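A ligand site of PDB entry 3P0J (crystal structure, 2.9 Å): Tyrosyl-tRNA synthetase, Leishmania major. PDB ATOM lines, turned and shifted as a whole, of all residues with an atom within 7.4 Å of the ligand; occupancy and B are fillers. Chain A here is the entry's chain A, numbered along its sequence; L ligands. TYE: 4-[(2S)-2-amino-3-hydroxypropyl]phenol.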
ATOM      1  N   TYR A  44      19.120  20.606 -27.341  1.00  0.00           N
ATOM      2  CA  TYR A  44      18.057  19.655 -27.147  1.00  0.00           C
ATOM      3  C   TYR A  44      16.714  20.344 -27.348  1.00  0.00           C
ATOM      4  O   TYR A  44      16.611  21.572 -27.310  1.00  0.00           O
ATOM      5  CB  TYR A  44      18.185  18.916 -25.802  1.00  0.00           C
ATOM      6  CG  TYR A  44      17.153  19.237 -24.733  1.00  0.00           C
ATOM      7  CD1 TYR A  44      16.143  18.339 -24.435  1.00  0.00           C
ATOM      8  CD2 TYR A  44      17.215  20.409 -24.004  1.00  0.00           C
ATOM      9  CE1 TYR A  44      15.223  18.608 -23.440  1.00  0.00           C
ATOM     10  CE2 TYR A  44      16.301  20.702 -23.029  1.00  0.00           C
ATOM     11  CZ  TYR A  44      15.296  19.800 -22.740  1.00  0.00           C
ATOM     12  OH  TYR A  44      14.378  20.107 -21.761  1.00  0.00           O
ATOM     13  N   ASP A  45      15.703  19.531 -27.601  1.00  0.00           N
ATOM     14  CA  ASP A  45      14.329  19.975 -27.616  1.00  0.00           C
ATOM     15  C   ASP A  45      13.525  18.728 -27.334  1.00  0.00           C
ATOM     16  O   ASP A  45      14.022  17.627 -27.572  1.00  0.00           O
ATOM     17  CB  ASP A  45      13.988  20.564 -28.984  1.00  0.00           C
ATOM     18  CG  ASP A  45      12.580  21.126 -29.036  1.00  0.00           C
ATOM     19  OD1 ASP A  45      11.951  21.340 -27.976  1.00  0.00           O
ATOM     20  OD2 ASP A  45      12.110  21.348 -30.165  1.00  0.00           O
ATOM     21  N   GLY A  46      12.303  18.857 -26.826  1.00  0.00           N
ATOM     22  CA  GLY A  46      11.545  17.671 -26.448  1.00  0.00           C
ATOM     23  C   GLY A  46      10.074  17.707 -26.806  1.00  0.00           C
ATOM     24  O   GLY A  46       9.519  18.772 -27.081  1.00  0.00           O
ATOM     25  N   PHE A  47       9.440  16.544 -26.805  1.00  0.00           N
ATOM     26  CA  PHE A  47       8.025  16.471 -27.104  1.00  0.00           C
ATOM     27  C   PHE A  47       7.331  15.178 -26.664  1.00  0.00           C
ATOM     28  O   PHE A  47       7.947  14.104 -26.649  1.00  0.00           O
ATOM     29  CB  PHE A  47       7.829  16.675 -28.604  1.00  0.00           C
ATOM     30  CG  PHE A  47       8.601  15.705 -29.446  1.00  0.00           C
ATOM     31  CD1 PHE A  47       7.992  14.563 -29.962  1.00  0.00           C
ATOM     32  CD2 PHE A  47       9.930  15.932 -29.753  1.00  0.00           C
ATOM     33  CE1 PHE A  47       8.699  13.660 -30.761  1.00  0.00           C
ATOM     34  CE2 PHE A  47      10.659  15.028 -30.551  1.00  0.00           C
ATOM     35  CZ  PHE A  47      10.037  13.898 -31.043  1.00  0.00           C
ATOM     36  N   GLU A  48       6.044  15.255 -26.330  1.00  0.00           N
ATOM     37  CA  GLU A  48       5.228  14.052 -26.150  1.00  0.00           C
ATOM     38  C   GLU A  48       4.566  13.747 -27.482  1.00  0.00           C
ATOM     39  O   GLU A  48       3.794  14.567 -27.971  1.00  0.00           O
ATOM     40  CB  GLU A  48       4.132  14.250 -25.095  1.00  0.00           C
ATOM     41  CG  GLU A  48       4.595  14.782 -23.748  1.00  0.00           C
ATOM     42  CD  GLU A  48       3.436  15.224 -22.870  1.00  0.00           C
ATOM     43  OE1 GLU A  48       2.798  14.342 -22.235  1.00  0.00           O
ATOM     44  OE2 GLU A  48       3.195  16.463 -22.853  1.00  0.00           O
ATOM     45  N   TRP A  78      14.572  14.897 -27.050  1.00  0.00           N
ATOM     46  CA  TRP A  78      14.149  14.157 -25.864  1.00  0.00           C
ATOM     47  C   TRP A  78      12.709  13.808 -26.096  1.00  0.00           C
ATOM     48  O   TRP A  78      11.873  14.691 -26.130  1.00  0.00           O
ATOM     49  CB  TRP A  78      14.288  15.034 -24.628  1.00  0.00           C
ATOM     50  CG  TRP A  78      13.972  14.336 -23.328  1.00  0.00           C
ATOM     51  CD1 TRP A  78      12.893  14.573 -22.506  1.00  0.00           C
ATOM     52  CD2 TRP A  78      14.737  13.299 -22.688  1.00  0.00           C
ATOM     53  NE1 TRP A  78      12.948  13.755 -21.400  1.00  0.00           N
ATOM     54  CE2 TRP A  78      14.061  12.959 -21.500  1.00  0.00           C
ATOM     55  CE3 TRP A  78      15.917  12.630 -23.011  1.00  0.00           C
ATOM     56  CZ2 TRP A  78      14.540  11.973 -20.636  1.00  0.00           C
ATOM     57  CZ3 TRP A  78      16.381  11.639 -22.138  1.00  0.00           C
ATOM     58  CH2 TRP A  78      15.695  11.328 -20.984  1.00  0.00           C
ATOM     59  N   VAL A  79      12.429  12.540 -26.280  1.00  0.00           N
ATOM     60  CA  VAL A  79      11.062  12.126 -26.526  1.00  0.00           C
ATOM     61  C   VAL A  79      10.429  11.829 -25.186  1.00  0.00           C
ATOM     62  O   VAL A  79      10.771  10.850 -24.550  1.00  0.00           O
ATOM     63  CB  VAL A  79      11.013  10.860 -27.414  1.00  0.00           C
ATOM     64  CG1 VAL A  79       9.592  10.438 -27.662  1.00  0.00           C
ATOM     65  CG2 VAL A  79      11.700  11.098 -28.733  1.00  0.00           C
ATOM     66  N   ALA A  80       9.522  12.674 -24.720  1.00  0.00           N
ATOM     67  CA  ALA A  80       8.904  12.460 -23.412  1.00  0.00           C
ATOM     68  C   ALA A  80       7.873  11.373 -23.495  1.00  0.00           C
ATOM     69  O   ALA A  80       6.682  11.660 -23.468  1.00  0.00           O
ATOM     70  CB  ALA A  80       8.248  13.737 -22.924  1.00  0.00           C
ATOM     71  N   PHE A  83       5.609   9.083 -19.743  1.00  0.00           N
ATOM     72  CA  PHE A  83       4.228   9.156 -19.261  1.00  0.00           C
ATOM     73  C   PHE A  83       3.293   8.092 -19.823  1.00  0.00           C
ATOM     74  O   PHE A  83       2.222   7.872 -19.288  1.00  0.00           O
ATOM     75  CB  PHE A  83       3.648  10.538 -19.514  1.00  0.00           C
ATOM     76  CG  PHE A  83       4.439  11.617 -18.891  1.00  0.00           C
ATOM     77  CD1 PHE A  83       4.408  11.794 -17.527  1.00  0.00           C
ATOM     78  CD2 PHE A  83       5.251  12.421 -19.652  1.00  0.00           C
ATOM     79  CE1 PHE A  83       5.153  12.780 -16.922  1.00  0.00           C
ATOM     80  CE2 PHE A  83       5.994  13.420 -19.067  1.00  0.00           C
ATOM     81  CZ  PHE A  83       5.958  13.592 -17.692  1.00  0.00           C
ATOM     82  N   SER A 123      12.781   8.902 -23.210  1.00  0.00           N
ATOM     83  CA  SER A 123      12.667   9.162 -21.796  1.00  0.00           C
ATOM     84  C   SER A 123      12.448   7.868 -21.039  1.00  0.00           C
ATOM     85  O   SER A 123      13.100   7.628 -20.023  1.00  0.00           O
ATOM     86  CB  SER A 123      11.509  10.119 -21.561  1.00  0.00           C
ATOM     87  OG  SER A 123      11.625  10.671 -20.269  1.00  0.00           O
ATOM     88  N   TYR A 134      18.581  10.597 -11.980  1.00  0.00           N
ATOM     89  CA  TYR A 134      17.481  11.399 -12.459  1.00  0.00           C
ATOM     90  C   TYR A 134      16.551  11.835 -11.313  1.00  0.00           C
ATOM     91  O   TYR A 134      16.490  13.015 -10.956  1.00  0.00           O
ATOM     92  CB  TYR A 134      16.679  10.630 -13.523  1.00  0.00           C
ATOM     93  CG  TYR A 134      15.566  11.448 -14.117  1.00  0.00           C
ATOM     94  CD1 TYR A 134      15.774  12.238 -15.223  1.00  0.00           C
ATOM     95  CD2 TYR A 134      14.294  11.447 -13.538  1.00  0.00           C
ATOM     96  CE1 TYR A 134      14.759  13.002 -15.774  1.00  0.00           C
ATOM     97  CE2 TYR A 134      13.270  12.219 -14.073  1.00  0.00           C
ATOM     98  CZ  TYR A 134      13.509  12.991 -15.190  1.00  0.00           C
ATOM     99  OH  TYR A 134      12.498  13.743 -15.720  1.00  0.00           O
ATOM    100  N   TYR A 171       5.641  18.032 -13.246  1.00  0.00           N
ATOM    101  CA  TYR A 171       6.058  18.030 -14.651  1.00  0.00           C
ATOM    102  C   TYR A 171       7.230  18.970 -14.903  1.00  0.00           C
ATOM    103  O   TYR A 171       8.199  18.559 -15.517  1.00  0.00           O
ATOM    104  CB  TYR A 171       4.897  18.328 -15.608  1.00  0.00           C
ATOM    105  CG  TYR A 171       3.739  17.345 -15.601  1.00  0.00           C
ATOM    106  CD1 TYR A 171       2.441  17.782 -15.793  1.00  0.00           C
ATOM    107  CD2 TYR A 171       3.936  15.995 -15.379  1.00  0.00           C
ATOM    108  CE1 TYR A 171       1.382  16.899 -15.766  1.00  0.00           C
ATOM    109  CE2 TYR A 171       2.881  15.108 -15.360  1.00  0.00           C
ATOM    110  CZ  TYR A 171       1.602  15.567 -15.552  1.00  0.00           C
ATOM    111  OH  TYR A 171       0.543  14.693 -15.529  1.00  0.00           O
ATOM    112  N   MET A 174      10.582  17.482 -13.440  1.00  0.00           N
ATOM    113  CA  MET A 174      11.063  16.472 -14.365  1.00  0.00           C
ATOM    114  C   MET A 174      11.684  17.112 -15.602  1.00  0.00           C
ATOM    115  O   MET A 174      12.821  16.799 -15.970  1.00  0.00           O
ATOM    116  CB  MET A 174       9.933  15.533 -14.773  1.00  0.00           C
ATOM    117  CG  MET A 174       9.511  14.584 -13.686  1.00  0.00           C
ATOM    118  SD  MET A 174       8.299  13.420 -14.294  1.00  0.00           S
ATOM    119  CE  MET A 174       6.897  14.461 -14.299  1.00  0.00           C
ATOM    120  N   GLN A 175      10.962  18.043 -16.229  1.00  0.00           N
ATOM    121  CA  GLN A 175      11.499  18.737 -17.404  1.00  0.00           C
ATOM    122  C   GLN A 175      12.807  19.423 -17.097  1.00  0.00           C
ATOM    123  O   GLN A 175      13.791  19.249 -17.816  1.00  0.00           O
ATOM    124  CB  GLN A 175      10.526  19.779 -17.964  1.00  0.00           C
ATOM    125  CG  GLN A 175      10.938  20.270 -19.371  1.00  0.00           C
ATOM    126  CD  GLN A 175       9.828  20.992 -20.104  1.00  0.00           C
ATOM    127  OE1 GLN A 175       8.657  20.925 -19.711  1.00  0.00           O
ATOM    128  NE2 GLN A 175      10.192  21.716 -21.165  1.00  0.00           N
ATOM    129  N   CYS A 176      12.817  20.222 -16.032  1.00  0.00           N
ATOM    130  CA  CYS A 176      14.011  20.940 -15.618  1.00  0.00           C
ATOM    131  C   CYS A 176      15.172  19.985 -15.354  1.00  0.00           C
ATOM    132  O   CYS A 176      16.327  20.357 -15.556  1.00  0.00           O
ATOM    133  CB  CYS A 176      13.744  21.774 -14.365  1.00  0.00           C
ATOM    134  SG  CYS A 176      15.137  22.807 -13.880  1.00  0.00           S
ATOM    135  N   CYS A 177      14.863  18.763 -14.918  1.00  0.00           N
ATOM    136  CA  CYS A 177      15.915  17.745 -14.711  1.00  0.00           C
ATOM    137  C   CYS A 177      16.516  17.278 -16.026  1.00  0.00           C
ATOM    138  O   CYS A 177      17.733  17.307 -16.202  1.00  0.00           O
ATOM    139  CB  CYS A 177      15.364  16.551 -13.951  1.00  0.00           C
ATOM    140  SG  CYS A 177      16.581  15.287 -13.682  1.00  0.00           S
ATOM    141  N   ASP A 178      15.649  16.871 -16.952  1.00  0.00           N
ATOM    142  CA  ASP A 178      16.050  16.482 -18.317  1.00  0.00           C
ATOM    143  C   ASP A 178      17.184  17.330 -18.832  1.00  0.00           C
ATOM    144  O   ASP A 178      18.159  16.816 -19.356  1.00  0.00           O
ATOM    145  CB  ASP A 178      14.890  16.627 -19.299  1.00  0.00           C
ATOM    146  CG  ASP A 178      13.697  15.770 -18.937  1.00  0.00           C
ATOM    147  OD1 ASP A 178      13.824  14.949 -18.025  1.00  0.00           O
ATOM    148  OD2 ASP A 178      12.626  15.929 -19.552  1.00  0.00           O
ATOM    149  N   ILE A 179      17.033  18.637 -18.673  1.00  0.00           N
ATOM    150  CA  ILE A 179      18.015  19.585 -19.184  1.00  0.00           C
ATOM    151  C   ILE A 179      19.422  19.241 -18.714  1.00  0.00           C
ATOM    152  O   ILE A 179      20.366  19.279 -19.507  1.00  0.00           O
ATOM    153  CB  ILE A 179      17.689  21.034 -18.780  1.00  0.00           C
ATOM    154  CG1 ILE A 179      16.316  21.446 -19.338  1.00  0.00           C
ATOM    155  CG2 ILE A 179      18.775  21.993 -19.276  1.00  0.00           C
ATOM    156  CD1 ILE A 179      16.027  22.927 -19.252  1.00  0.00           C
ATOM    157  N   LEU A 182      20.616  15.241 -19.783  1.00  0.00           N
ATOM    158  CA  LEU A 182      21.177  15.175 -21.139  1.00  0.00           C
ATOM    159  C   LEU A 182      22.439  15.984 -21.327  1.00  0.00           C
ATOM    160  O   LEU A 182      23.107  15.839 -22.349  1.00  0.00           O
ATOM    161  CB  LEU A 182      20.170  15.737 -22.147  1.00  0.00           C
ATOM    162  CG  LEU A 182      19.005  14.846 -22.499  1.00  0.00           C
ATOM    163  CD1 LEU A 182      18.050  15.624 -23.383  1.00  0.00           C
ATOM    164  CD2 LEU A 182      19.513  13.615 -23.203  1.00  0.00           C
ATOM    165  N   LEU A 189      13.977  25.168 -27.491  1.00  0.00           N
ATOM    166  CA  LEU A 189      12.552  24.845 -27.440  1.00  0.00           C
ATOM    167  C   LEU A 189      11.719  26.076 -27.726  1.00  0.00           C
ATOM    168  O   LEU A 189      12.226  27.197 -27.891  1.00  0.00           O
ATOM    169  CB  LEU A 189      12.169  24.292 -26.073  1.00  0.00           C
ATOM    170  CG  LEU A 189      12.989  23.140 -25.509  1.00  0.00           C
ATOM    171  CD1 LEU A 189      14.234  23.672 -24.890  1.00  0.00           C
ATOM    172  CD2 LEU A 189      12.174  22.349 -24.494  1.00  0.00           C
ATOM    173  N   ASP A 192       7.219  29.282 -25.349  1.00  0.00           N
ATOM    174  CA  ASP A 192       6.339  29.006 -24.245  1.00  0.00           C
ATOM    175  C   ASP A 192       6.946  28.071 -23.221  1.00  0.00           C
ATOM    176  O   ASP A 192       6.415  27.984 -22.110  1.00  0.00           O
ATOM    177  CB  ASP A 192       4.953  28.530 -24.733  1.00  0.00           C
ATOM    178  CG  ASP A 192       4.943  27.125 -25.359  1.00  0.00           C
ATOM    179  OD1 ASP A 192       5.997  26.574 -25.734  1.00  0.00           O
ATOM    180  OD2 ASP A 192       3.839  26.565 -25.500  1.00  0.00           O
ATOM    181  N   GLN A 193       8.062  27.394 -23.525  1.00  0.00           N
ATOM    182  CA  GLN A 193       8.769  26.597 -22.498  1.00  0.00           C
ATOM    183  C   GLN A 193       9.753  27.456 -21.674  1.00  0.00           C
ATOM    184  O   GLN A 193      10.499  26.945 -20.837  1.00  0.00           O
ATOM    185  CB  GLN A 193       9.561  25.449 -23.095  1.00  0.00           C
ATOM    186  CG  GLN A 193       8.868  24.638 -24.140  1.00  0.00           C
ATOM    187  CD  GLN A 193       7.595  24.040 -23.649  1.00  0.00           C
ATOM    188  OE1 GLN A 193       7.567  22.896 -23.192  1.00  0.00           O
ATOM    189  NE2 GLN A 193       6.518  24.800 -23.747  1.00  0.00           N
ATOM    190  N   VAL A 196      10.384  27.094 -17.568  1.00  0.00           N
ATOM    191  CA  VAL A 196      11.061  25.867 -17.172  1.00  0.00           C
ATOM    192  C   VAL A 196      12.549  25.978 -17.471  1.00  0.00           C
ATOM    193  O   VAL A 196      13.366  25.708 -16.622  1.00  0.00           O
ATOM    194  CB  VAL A 196      10.498  24.642 -17.871  1.00  0.00           C
ATOM    195  CG1 VAL A 196      11.156  23.380 -17.357  1.00  0.00           C
ATOM    196  CG2 VAL A 196       8.995  24.565 -17.646  1.00  0.00           C
ATOM    197  N   ASN A 197      12.885  26.407 -18.680  1.00  0.00           N
ATOM    198  CA  ASN A 197      14.282  26.603 -19.071  1.00  0.00           C
ATOM    199  C   ASN A 197      14.984  27.601 -18.173  1.00  0.00           C
ATOM    200  O   ASN A 197      16.082  27.364 -17.680  1.00  0.00           O
ATOM    201  CB  ASN A 197      14.392  27.025 -20.529  1.00  0.00           C
ATOM    202  CG  ASN A 197      14.092  25.884 -21.493  1.00  0.00           C
ATOM    203  OD1 ASN A 197      14.590  24.770 -21.339  1.00  0.00           O
ATOM    204  ND2 ASN A 197      13.276  26.158 -22.505  1.00  0.00           N
HETATM  205  C   TYE L   1       5.332  19.850 -23.722  1.00  0.00           C
HETATM  206  N   TYE L   1       6.858  20.109 -21.846  1.00  0.00           N
HETATM  207  O   TYE L   1       4.652  18.885 -22.859  1.00  0.00           O
HETATM  208  CA  TYE L   1       6.827  19.963 -23.322  1.00  0.00           C
HETATM  209  CB  TYE L   1       7.556  18.697 -23.823  1.00  0.00           C
HETATM  210  CG  TYE L   1       8.941  18.463 -23.207  1.00  0.00           C
HETATM  211  OH  TYE L   1      12.656  17.785 -21.567  1.00  0.00           O
HETATM  212  CZ  TYE L   1      11.453  18.015 -22.117  1.00  0.00           C
HETATM  213  CD1 TYE L   1       9.098  17.461 -22.254  1.00  0.00           C
HETATM  214  CD2 TYE L   1      10.027  19.219 -23.617  1.00  0.00           C
HETATM  215  CE1 TYE L   1      10.357  17.258 -21.710  1.00  0.00           C
HETATM  216  CE2 TYE L   1      11.286  19.006 -23.070  1.00  0.00           C
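O of Gly 46 touches CD2 of the ligand, at 3.5 Å.
Phe 47 touches the ligand.
CD1 of Trp 78 touches OH of the ligand, 3.4 Å away.
Ala 80 touches the ligand (CB to CD1, 3.9 Å).
Leu 189 touches the ligand (CD2 to CE2, 3.7 Å).
Of the 24 residues printed, 10 come within 4 Å of the ligand.
Along chain A the residues within 4 Å of the ligand span positions 44 to 193.
An oxygen (OH) of the ligand sits at hydrogen-bond distance from the side-chain hydroxyl of Tyr 44, at 2.9 Å.
OH of the ligand lies within hydrogen-bond range of OD2 of Asp 178.
OE1 of Gln 193 sits close to N of the ligand, 3.2 Å away.
The side-chain amide oxygen (OE1) of Gln 175 is in hydrogen-bond range of a nitrogen (N) of the ligand (2.9 Å).
The side-chain carboxylate of Glu 48 lies within hydrogen-bond range of an oxygen (O) of the ligand (2.8 Å).
O of Phe 47 sits at hydrogen-bond distance from N of Ala 80, 2.9 Å away.
O of Gln 193 lies within hydrogen-bond range of ND2 of Asn 197.
The side-chain amide nitrogen (NE2) of Gln 193 is in hydrogen-bond range of the side-chain carboxylate (OD1) of Asp 192.
The backbone carbonyl oxygen (O) of Trp 78 lies within hydrogen-bond range of the backbone NH (N) of Phe 47 (3.1 Å).
O of Asp 45 sits at hydrogen-bond distance from N of Trp 78, at 2.8 Å.
The side-chain hydroxyl (OH) of Tyr 134 sits at hydrogen-bond distance from the side-chain carboxylate (OD1) of Asp 178 (2.9 Å).
OD2 of Asp 178 is in hydrogen-bond range of NE1 of Trp 78, 2.9 Å away.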
